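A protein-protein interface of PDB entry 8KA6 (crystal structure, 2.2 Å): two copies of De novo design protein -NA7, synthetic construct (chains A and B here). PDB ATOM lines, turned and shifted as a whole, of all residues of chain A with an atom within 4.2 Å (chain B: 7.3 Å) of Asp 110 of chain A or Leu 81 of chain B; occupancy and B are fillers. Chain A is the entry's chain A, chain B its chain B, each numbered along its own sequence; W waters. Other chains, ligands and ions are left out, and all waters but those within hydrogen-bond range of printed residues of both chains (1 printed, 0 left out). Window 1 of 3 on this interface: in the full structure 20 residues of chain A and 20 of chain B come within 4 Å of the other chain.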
ATOM      1  N   ARG A 106     -38.036 -15.022  18.909  1.00  0.00           N
ATOM      2  CA  ARG A 106     -37.246 -14.209  19.828  1.00  0.00           C
ATOM      3  C   ARG A 106     -35.982 -14.940  20.259  1.00  0.00           C
ATOM      4  O   ARG A 106     -34.891 -14.358  20.275  1.00  0.00           O
ATOM      5  CB  ARG A 106     -38.088 -13.828  21.045  1.00  0.00           C
ATOM      6  CG  ARG A 106     -37.319 -13.082  22.121  1.00  0.00           C
ATOM      7  CD  ARG A 106     -36.676 -11.822  21.565  1.00  0.00           C
ATOM      8  NE  ARG A 106     -36.275 -10.902  22.621  1.00  0.00           N
ATOM      9  CZ  ARG A 106     -37.051  -9.945  23.111  1.00  0.00           C
ATOM     10  NH1 ARG A 106     -38.277  -9.748  22.653  1.00  0.00           N
ATOM     11  NH2 ARG A 106     -36.585  -9.165  24.082  1.00  0.00           N
ATOM     12  N   GLU A 107     -36.109 -16.219  20.620  1.00  0.00           N
ATOM     13  CA  GLU A 107     -34.937 -16.989  21.023  1.00  0.00           C
ATOM     14  C   GLU A 107     -33.968 -17.161  19.862  1.00  0.00           C
ATOM     15  O   GLU A 107     -32.748 -17.107  20.049  1.00  0.00           O
ATOM     16  CB  GLU A 107     -35.365 -18.348  21.574  1.00  0.00           C
ATOM     17  CG  GLU A 107     -36.181 -18.267  22.852  1.00  0.00           C
ATOM     18  CD  GLU A 107     -36.597 -19.631  23.365  1.00  0.00           C
ATOM     19  OE1 GLU A 107     -36.317 -20.635  22.678  1.00  0.00           O
ATOM     20  OE2 GLU A 107     -37.205 -19.698  24.453  1.00  0.00           O
ATOM     21  N   ALA A 108     -34.495 -17.364  18.652  1.00  0.00           N
ATOM     22  CA  ALA A 108     -33.626 -17.506  17.488  1.00  0.00           C
ATOM     23  C   ALA A 108     -32.912 -16.200  17.171  1.00  0.00           C
ATOM     24  O   ALA A 108     -31.726 -16.203  16.824  1.00  0.00           O
ATOM     25  CB  ALA A 108     -34.435 -17.988  16.283  1.00  0.00           C
ATOM     26  N   ALA A 109     -33.617 -15.071  17.290  1.00  0.00           N
ATOM     27  CA  ALA A 109     -32.984 -13.779  17.045  1.00  0.00           C
ATOM     28  C   ALA A 109     -31.935 -13.469  18.104  1.00  0.00           C
ATOM     29  O   ALA A 109     -30.889 -12.885  17.797  1.00  0.00           O
ATOM     30  CB  ALA A 109     -34.042 -12.676  16.995  1.00  0.00           C
ATOM     31  N   ASP A 110     -32.196 -13.851  19.357  1.00  0.00           N
ATOM     32  CA  ASP A 110     -31.219 -13.619  20.417  1.00  0.00           C
ATOM     33  C   ASP A 110     -29.984 -14.492  20.232  1.00  0.00           C
ATOM     34  O   ASP A 110     -28.854 -14.024  20.416  1.00  0.00           O
ATOM     35  CB  ASP A 110     -31.855 -13.871  21.785  1.00  0.00           C
ATOM     36  CG  ASP A 110     -32.759 -12.735  22.226  1.00  0.00           C
ATOM     37  OD1 ASP A 110     -32.813 -11.708  21.517  1.00  0.00           O
ATOM     38  OD2 ASP A 110     -33.413 -12.867  23.283  1.00  0.00           O
ATOM     39  N   ARG A 111     -30.177 -15.764  19.874  1.00  0.00           N
ATOM     40  CA  ARG A 111     -29.033 -16.634  19.621  1.00  0.00           C
ATOM     41  C   ARG A 111     -28.209 -16.128  18.446  1.00  0.00           C
ATOM     42  O   ARG A 111     -26.974 -16.118  18.504  1.00  0.00           O
ATOM     43  CB  ARG A 111     -29.502 -18.069  19.375  1.00  0.00           C
ATOM     44  CG  ARG A 111     -28.439 -18.964  18.755  1.00  0.00           C
ATOM     45  CD  ARG A 111     -28.556 -20.404  19.226  1.00  0.00           C
ATOM     46  NE  ARG A 111     -28.318 -20.527  20.660  1.00  0.00           N
ATOM     47  CZ  ARG A 111     -28.041 -21.665  21.281  1.00  0.00           C
ATOM     48  NH1 ARG A 111     -27.940 -22.807  20.619  1.00  0.00           N
ATOM     49  NH2 ARG A 111     -27.855 -21.657  22.598  1.00  0.00           N
ATOM     50  N   LEU A 112     -28.876 -15.692  17.374  1.00  0.00           N
ATOM     51  CA  LEU A 112     -28.155 -15.146  16.230  1.00  0.00           C
ATOM     52  C   LEU A 112     -27.389 -13.886  16.615  1.00  0.00           C
ATOM     53  O   LEU A 112     -26.283 -13.645  16.117  1.00  0.00           O
ATOM     54  CB  LEU A 112     -29.127 -14.861  15.086  1.00  0.00           C
ATOM     55  CG  LEU A 112     -28.516 -14.318  13.794  1.00  0.00           C
ATOM     56  CD1 LEU A 112     -27.476 -15.285  13.246  1.00  0.00           C
ATOM     57  CD2 LEU A 112     -29.598 -14.048  12.762  1.00  0.00           C
ATOM     58  N   ARG A 113     -27.962 -13.072  17.504  1.00  0.00           N
ATOM     59  CA  ARG A 113     -27.256 -11.888  17.982  1.00  0.00           C
ATOM     60  C   ARG A 113     -26.023 -12.271  18.789  1.00  0.00           C
ATOM     61  O   ARG A 113     -24.973 -11.629  18.672  1.00  0.00           O
ATOM     62  CB  ARG A 113     -28.194 -11.020  18.821  1.00  0.00           C
ATOM     63  CG  ARG A 113     -27.592  -9.687  19.237  1.00  0.00           C
ATOM     64  CD  ARG A 113     -27.583  -8.713  18.070  1.00  0.00           C
ATOM     65  NE  ARG A 113     -26.368  -7.911  18.026  1.00  0.00           N
ATOM     66  CZ  ARG A 113     -26.135  -6.959  17.133  1.00  0.00           C
ATOM     67  NH1 ARG A 113     -27.027  -6.648  16.207  1.00  0.00           N
ATOM     68  NH2 ARG A 113     -24.980  -6.302  17.171  1.00  0.00           N
ATOM     69  N   ALA A 114     -26.132 -13.315  19.614  1.00  0.00           N
ATOM     70  CA  ALA A 114     -24.997 -13.738  20.426  1.00  0.00           C
ATOM     71  C   ALA A 114     -23.873 -14.293  19.560  1.00  0.00           C
ATOM     72  O   ALA A 114     -22.692 -14.066  19.848  1.00  0.00           O
ATOM     73  CB  ALA A 114     -25.448 -14.773  21.455  1.00  0.00           C
ATOM     74  N   ARG B  49     -33.656  -1.217  21.844  1.00  0.00           N
ATOM     75  CA  ARG B  49     -33.050  -2.518  21.580  1.00  0.00           C
ATOM     76  C   ARG B  49     -31.742  -2.371  20.814  1.00  0.00           C
ATOM     77  O   ARG B  49     -30.765  -3.069  21.108  1.00  0.00           O
ATOM     78  CB  ARG B  49     -34.025  -3.405  20.807  1.00  0.00           C
ATOM     79  CG  ARG B  49     -35.205  -3.898  21.626  1.00  0.00           C
ATOM     80  CD  ARG B  49     -36.201  -4.637  20.750  1.00  0.00           C
ATOM     81  NE  ARG B  49     -37.318  -5.168  21.520  1.00  0.00           N
ATOM     82  CZ  ARG B  49     -38.424  -5.668  20.987  1.00  0.00           C
ATOM     83  NH1 ARG B  49     -38.601  -5.711  19.676  1.00  0.00           N
ATOM     84  NH2 ARG B  49     -39.379  -6.131  21.788  1.00  0.00           N
ATOM     85  N   ALA B  52     -29.194  -1.445  23.221  1.00  0.00           N
ATOM     86  CA  ALA B  52     -28.732  -2.592  23.996  1.00  0.00           C
ATOM     87  C   ALA B  52     -27.756  -3.444  23.195  1.00  0.00           C
ATOM     88  O   ALA B  52     -26.784  -3.971  23.750  1.00  0.00           O
ATOM     89  CB  ALA B  52     -29.923  -3.431  24.454  1.00  0.00           C
ATOM     90  N   ASP B  53     -28.000  -3.598  21.889  1.00  0.00           N
ATOM     91  CA  ASP B  53     -27.040  -4.300  21.042  1.00  0.00           C
ATOM     92  C   ASP B  53     -25.726  -3.535  20.943  1.00  0.00           C
ATOM     93  O   ASP B  53     -24.660  -4.148  20.810  1.00  0.00           O
ATOM     94  CB  ASP B  53     -27.626  -4.532  19.648  1.00  0.00           C
ATOM     95  CG  ASP B  53     -28.729  -5.572  19.644  1.00  0.00           C
ATOM     96  OD1 ASP B  53     -28.809  -6.357  20.613  1.00  0.00           O
ATOM     97  OD2 ASP B  53     -29.510  -5.613  18.670  1.00  0.00           O
ATOM     98  N   ILE B  56     -23.768  -4.092  24.306  1.00  0.00           N
ATOM     99  CA  ILE B  56     -23.162  -5.417  24.393  1.00  0.00           C
ATOM    100  C   ILE B  56     -21.898  -5.486  23.543  1.00  0.00           C
ATOM    101  O   ILE B  56     -20.895  -6.086  23.947  1.00  0.00           O
ATOM    102  CB  ILE B  56     -24.189  -6.491  23.990  1.00  0.00           C
ATOM    103  CG1 ILE B  56     -25.290  -6.585  25.048  1.00  0.00           C
ATOM    104  CG2 ILE B  56     -23.514  -7.842  23.782  1.00  0.00           C
ATOM    105  CD1 ILE B  56     -26.380  -7.568  24.710  1.00  0.00           C
ATOM    106  N   ALA B  74     -20.363 -16.532  23.077  1.00  0.00           N
ATOM    107  CA  ALA B  74     -21.699 -16.603  22.491  1.00  0.00           C
ATOM    108  C   ALA B  74     -22.722 -17.071  23.515  1.00  0.00           C
ATOM    109  O   ALA B  74     -23.842 -16.549  23.571  1.00  0.00           O
ATOM    110  CB  ALA B  74     -21.694 -17.527  21.273  1.00  0.00           C
ATOM    111  N   ALA B  75     -22.357 -18.057  24.338  1.00  0.00           N
ATOM    112  CA  ALA B  75     -23.235 -18.463  25.428  1.00  0.00           C
ATOM    113  C   ALA B  75     -23.342 -17.377  26.490  1.00  0.00           C
ATOM    114  O   ALA B  75     -24.375 -17.266  27.161  1.00  0.00           O
ATOM    115  CB  ALA B  75     -22.737 -19.769  26.048  1.00  0.00           C
ATOM    116  N   LEU B  76     -22.293 -16.567  26.652  1.00  0.00           N
ATOM    117  CA  LEU B  76     -22.336 -15.486  27.631  1.00  0.00           C
ATOM    118  C   LEU B  76     -23.277 -14.376  27.183  1.00  0.00           C
ATOM    119  O   LEU B  76     -24.062 -13.856  27.985  1.00  0.00           O
ATOM    120  CB  LEU B  76     -20.928 -14.935  27.862  1.00  0.00           C
ATOM    121  CG  LEU B  76     -20.649 -14.311  29.230  1.00  0.00           C
ATOM    122  CD1 LEU B  76     -20.433 -15.398  30.275  1.00  0.00           C
ATOM    123  CD2 LEU B  76     -19.455 -13.369  29.168  1.00  0.00           C
ATOM    124  N   VAL B  77     -23.211 -13.998  25.904  1.00  0.00           N
ATOM    125  CA  VAL B  77     -24.098 -12.963  25.383  1.00  0.00           C
ATOM    126  C   VAL B  77     -25.535 -13.464  25.334  1.00  0.00           C
ATOM    127  O   VAL B  77     -26.481 -12.708  25.589  1.00  0.00           O
ATOM    128  CB  VAL B  77     -23.612 -12.497  23.998  1.00  0.00           C
ATOM    129  CG1 VAL B  77     -24.550 -11.446  23.422  1.00  0.00           C
ATOM    130  CG2 VAL B  77     -22.193 -11.960  24.088  1.00  0.00           C
ATOM    131  N   GLU B  78     -25.726 -14.746  25.011  1.00  0.00           N
ATOM    132  CA  GLU B  78     -27.074 -15.297  24.959  1.00  0.00           C
ATOM    133  C   GLU B  78     -27.715 -15.341  26.340  1.00  0.00           C
ATOM    134  O   GLU B  78     -28.943 -15.247  26.455  1.00  0.00           O
ATOM    135  CB  GLU B  78     -27.047 -16.693  24.338  1.00  0.00           C
ATOM    136  CG  GLU B  78     -28.413 -17.202  23.915  1.00  0.00           C
ATOM    137  CD  GLU B  78     -28.344 -18.563  23.257  1.00  0.00           C
ATOM    138  OE1 GLU B  78     -27.254 -19.173  23.268  1.00  0.00           O
ATOM    139  OE2 GLU B  78     -29.377 -19.022  22.727  1.00  0.00           O
ATOM    140  N   ARG B  79     -26.908 -15.479  27.395  1.00  0.00           N
ATOM    141  CA  ARG B  79     -27.447 -15.397  28.749  1.00  0.00           C
ATOM    142  C   ARG B  79     -27.773 -13.959  29.129  1.00  0.00           C
ATOM    143  O   ARG B  79     -28.640 -13.724  29.978  1.00  0.00           O
ATOM    144  CB  ARG B  79     -26.460 -16.002  29.747  1.00  0.00           C
ATOM    145  N   LEU B  80     -27.090 -12.990  28.516  1.00  0.00           N
ATOM    146  CA  LEU B  80     -27.404 -11.586  28.760  1.00  0.00           C
ATOM    147  C   LEU B  80     -28.688 -11.179  28.048  1.00  0.00           C
ATOM    148  O   LEU B  80     -29.525 -10.469  28.620  1.00  0.00           O
ATOM    149  CB  LEU B  80     -26.237 -10.705  28.311  1.00  0.00           C
ATOM    150  CG  LEU B  80     -25.190 -10.290  29.350  1.00  0.00           C
ATOM    151  CD1 LEU B  80     -25.751  -9.215  30.267  1.00  0.00           C
ATOM    152  CD2 LEU B  80     -24.695 -11.482  30.158  1.00  0.00           C
ATOM    153  N   LEU B  81     -28.863 -11.622  26.799  1.00  0.00           N
ATOM    154  CA  LEU B  81     -30.052 -11.258  26.035  1.00  0.00           C
ATOM    155  C   LEU B  81     -31.307 -11.924  26.584  1.00  0.00           C
ATOM    156  O   LEU B  81     -32.408 -11.384  26.430  1.00  0.00           O
ATOM    157  CB  LEU B  81     -29.860 -11.630  24.564  1.00  0.00           C
ATOM    158  CG  LEU B  81     -28.807 -10.848  23.777  1.00  0.00           C
ATOM    159  CD1 LEU B  81     -28.540 -11.511  22.438  1.00  0.00           C
ATOM    160  CD2 LEU B  81     -29.256  -9.412  23.578  1.00  0.00           C
ATOM    161  N   ALA B  82     -31.167 -13.084  27.220  1.00  0.00           N
ATOM    162  CA  ALA B  82     -32.322 -13.814  27.716  1.00  0.00           C
ATOM    163  C   ALA B  82     -32.922 -13.112  28.934  1.00  0.00           C
ATOM    164  O   ALA B  82     -32.370 -12.147  29.473  1.00  0.00           O
ATOM    165  CB  ALA B  82     -31.936 -15.250  28.069  1.00  0.00           C
ATOM    166  N   GLY B  83     -34.080 -13.615  29.367  1.00  0.00           N
ATOM    167  CA  GLY B  83     -34.739 -13.069  30.540  1.00  0.00           C
ATOM    168  C   GLY B  83     -33.971 -13.272  31.829  1.00  0.00           C
ATOM    169  O   GLY B  83     -34.232 -12.568  32.809  1.00  0.00           O
ATOM    170  N   THR B  84     -33.032 -14.221  31.851  1.00  0.00           N
ATOM    171  CA  THR B  84     -32.206 -14.422  33.036  1.00  0.00           C
ATOM    172  C   THR B  84     -31.339 -13.199  33.307  1.00  0.00           C
ATOM    173  O   THR B  84     -31.338 -12.658  34.419  1.00  0.00           O
ATOM    174  CB  THR B  84     -31.339 -15.670  32.868  1.00  0.00           C
ATOM    175  N   GLY B  85     -30.603 -12.743  32.294  1.00  0.00           N
ATOM    176  CA  GLY B  85     -29.753 -11.576  32.428  1.00  0.00           C
ATOM    177  C   GLY B  85     -28.711 -11.721  33.517  1.00  0.00           C
ATOM    178  O   GLY B  85     -28.609 -10.869  34.404  1.00  0.00           O
ATOM    179  N   GLU B  86     -27.940 -12.802  33.465  1.00  0.00           N
ATOM    180  CA  GLU B  86     -26.926 -13.082  34.479  1.00  0.00           C
ATOM    181  C   GLU B  86     -25.646 -12.353  34.095  1.00  0.00           C
ATOM    182  O   GLU B  86     -24.923 -12.776  33.189  1.00  0.00           O
ATOM    183  CB  GLU B  86     -26.698 -14.584  34.610  1.00  0.00           C
ATOM    184  N   ALA B 102     -27.626  -2.728  29.423  1.00  0.00           N
ATOM    185  CA  ALA B 102     -28.186  -3.362  28.235  1.00  0.00           C
ATOM    186  C   ALA B 102     -29.394  -4.219  28.588  1.00  0.00           C
ATOM    187  O   ALA B 102     -30.385  -4.241  27.848  1.00  0.00           O
ATOM    188  CB  ALA B 102     -27.117  -4.196  27.530  1.00  0.00           C
ATOM    189  N   VAL B 103     -29.331  -4.930  29.717  1.00  0.00           N
ATOM    190  CA  VAL B 103     -30.481  -5.701  30.177  1.00  0.00           C
ATOM    191  C   VAL B 103     -31.613  -4.774  30.598  1.00  0.00           C
ATOM    192  O   VAL B 103     -32.790  -5.046  30.333  1.00  0.00           O
ATOM    193  CB  VAL B 103     -30.065  -6.645  31.321  1.00  0.00           C
ATOM    194  CG1 VAL B 103     -31.278  -7.366  31.890  1.00  0.00           C
ATOM    195  CG2 VAL B 103     -29.030  -7.645  30.834  1.00  0.00           C
ATOM    196  N   ARG B 106     -33.329  -3.522  27.466  1.00  0.00           N
ATOM    197  CA  ARG B 106     -34.127  -4.558  26.815  1.00  0.00           C
ATOM    198  C   ARG B 106     -35.377  -4.886  27.619  1.00  0.00           C
ATOM    199  O   ARG B 106     -36.462  -5.052  27.049  1.00  0.00           O
ATOM    200  CB  ARG B 106     -33.284  -5.814  26.594  1.00  0.00           C
ATOM    201  CG  ARG B 106     -32.406  -5.757  25.356  1.00  0.00           C
ATOM    202  CD  ARG B 106     -31.493  -6.969  25.255  1.00  0.00           C
ATOM    203  NE  ARG B 106     -32.240  -8.219  25.182  1.00  0.00           N
ATOM    204  CZ  ARG B 106     -32.684  -8.763  24.056  1.00  0.00           C
ATOM    205  NH1 ARG B 106     -32.489  -8.182  22.884  1.00  0.00           N
ATOM    206  NH2 ARG B 106     -33.340  -9.918  24.110  1.00  0.00           N
ATOM    207  N   ASP B 110     -39.149  -4.431  26.226  1.00  0.00           N
ATOM    208  CA  ASP B 110     -40.187  -5.458  26.203  1.00  0.00           C
ATOM    209  C   ASP B 110     -41.417  -5.016  26.984  1.00  0.00           C
ATOM    210  O   ASP B 110     -42.552  -5.293  26.578  1.00  0.00           O
ATOM    211  CB  ASP B 110     -39.645  -6.772  26.766  1.00  0.00           C
ATOM    212  CG  ASP B 110     -38.760  -7.509  25.781  1.00  0.00           C
ATOM    213  OD1 ASP B 110     -38.610  -7.035  24.635  1.00  0.00           O
ATOM    214  OD2 ASP B 110     -38.212  -8.567  26.158  1.00  0.00           O
HETATM  215  O   HOH W   1     -24.264  -6.721  19.953  1.00  0.00           O
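Water W1 bridges the backbone carbonyl oxygen of Asp 53 of chain B (2.7 Å) and the guanidinium group of Arg 113 of chain A (2.9 Å).
NE of Arg 106 of chain A lies within salt-bridge range of OD2 of Asp 110 of chain A (3.5 Å). NH2 of Arg 49 of chain B is in salt-bridge range of OD1 of Asp 110 of chain B, 3.1 Å away. The backbone carbonyl oxygen (O) of Leu 81 of chain B is in hydrogen-bond range of the guanidinium group (NH2) of Arg 106 of chain B, at 2.9 Å.
Hydrophobic or aromatic side chains of chain B that line the printed part of chain A: Ala 74, Val 77 and Leu 81. Printed residues of chain A that touch a printed residue of chain B: Arg 106, Asp 110, Arg 111, Arg 113 and Ala 114. Hydrophobic or aromatic side chains of chain A within 4 Å of the printed part of chain B: Ala 114. Among the printed residues, 11 pairs touch across the chains. Among the printed residues, Asp or Glu carboxylates within 4 Å of a Lys or Arg side-chain nitrogen of the other chain: Arg 106 of chain A with Asp 110 of chain B, Asp 110 of chain A with Arg 106 of chain B, Arg 111 of chain A with Glu 78 of chain B and Arg 113 of chain A with Asp 53 of chain B.
Arg 106 of chain A touches its own counterpart, Arg 106 of chain B. Arg 106 of chain A touches Asp 110 of chain B, and with the chains exchanged Asp 110 of chain A touches Arg 106 of chain B. 2 positions are printed for both chains. Of the 11 pairs that touch across the chains among the printed residues, 3 have their exchanged pair printed and touching as well.
The guanidinium group (NH1) of Arg 113 of chain A is in salt-bridge range of the side-chain carboxylate (OD2) of Asp 53 of chain B (3.6 Å). OD2 of Asp 110 of chain A lies within salt-bridge range of NH2 of Arg 106 of chain B (3.1 Å). NH2 of Arg 106 of chain A sits close to NH2 of Arg 106 of chain B, at 3.3 Å. OD2 of Asp 110 of chain B is in salt-bridge range of NH2 of Arg 106 of chain A (2.7 Å). The guanidinium group (NH2) of Arg 111 of chain A lies within salt-bridge range of the side-chain carboxylate (OE1) of Glu 78 of chain B, 2.6 Å away.
NH1 of Arg 106 of chain A touches NH2 of Arg 49 of chain B (3.9 Å). O of Asp 110 of chain A touches CD1 of Leu 81 of chain B, 3.2 Å away. CD1 of Leu 81 of chain B touches CB of Arg 113 of chain A, at 3.7 Å. O of Ala 74 of chain B touches CB of Ala 114 of chain A (3.2 Å). Ala 114 of chain A touches Val 77 of chain B. Glu 78 of chain B touches Ala 114 of chain A.
Ala 109 of chain A touches none of the printed residues of chain B. Of chain B, only Leu 81 (3.2 Å) and Arg 106 (3.1 Å) come within 4 Å of Asp 110 of chain A. Of the printed residues of chain B, Arg 113 of chain A touches Asp 53 and Leu 81. Of the printed residues of chain A, Val 77 of chain B touches Ala 114 (3.8 Å). Printed residues of chain A within 4 Å of Glu 78 of chain B: Arg 111 (2.6 Å) and Ala 114 (3.6 Å). Thr 84 of chain B touches none of the printed residues of chain A. The nearest residue of chain B that does not touch Asp 110 of chain A is Ala 82 of chain B (4.5 Å).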
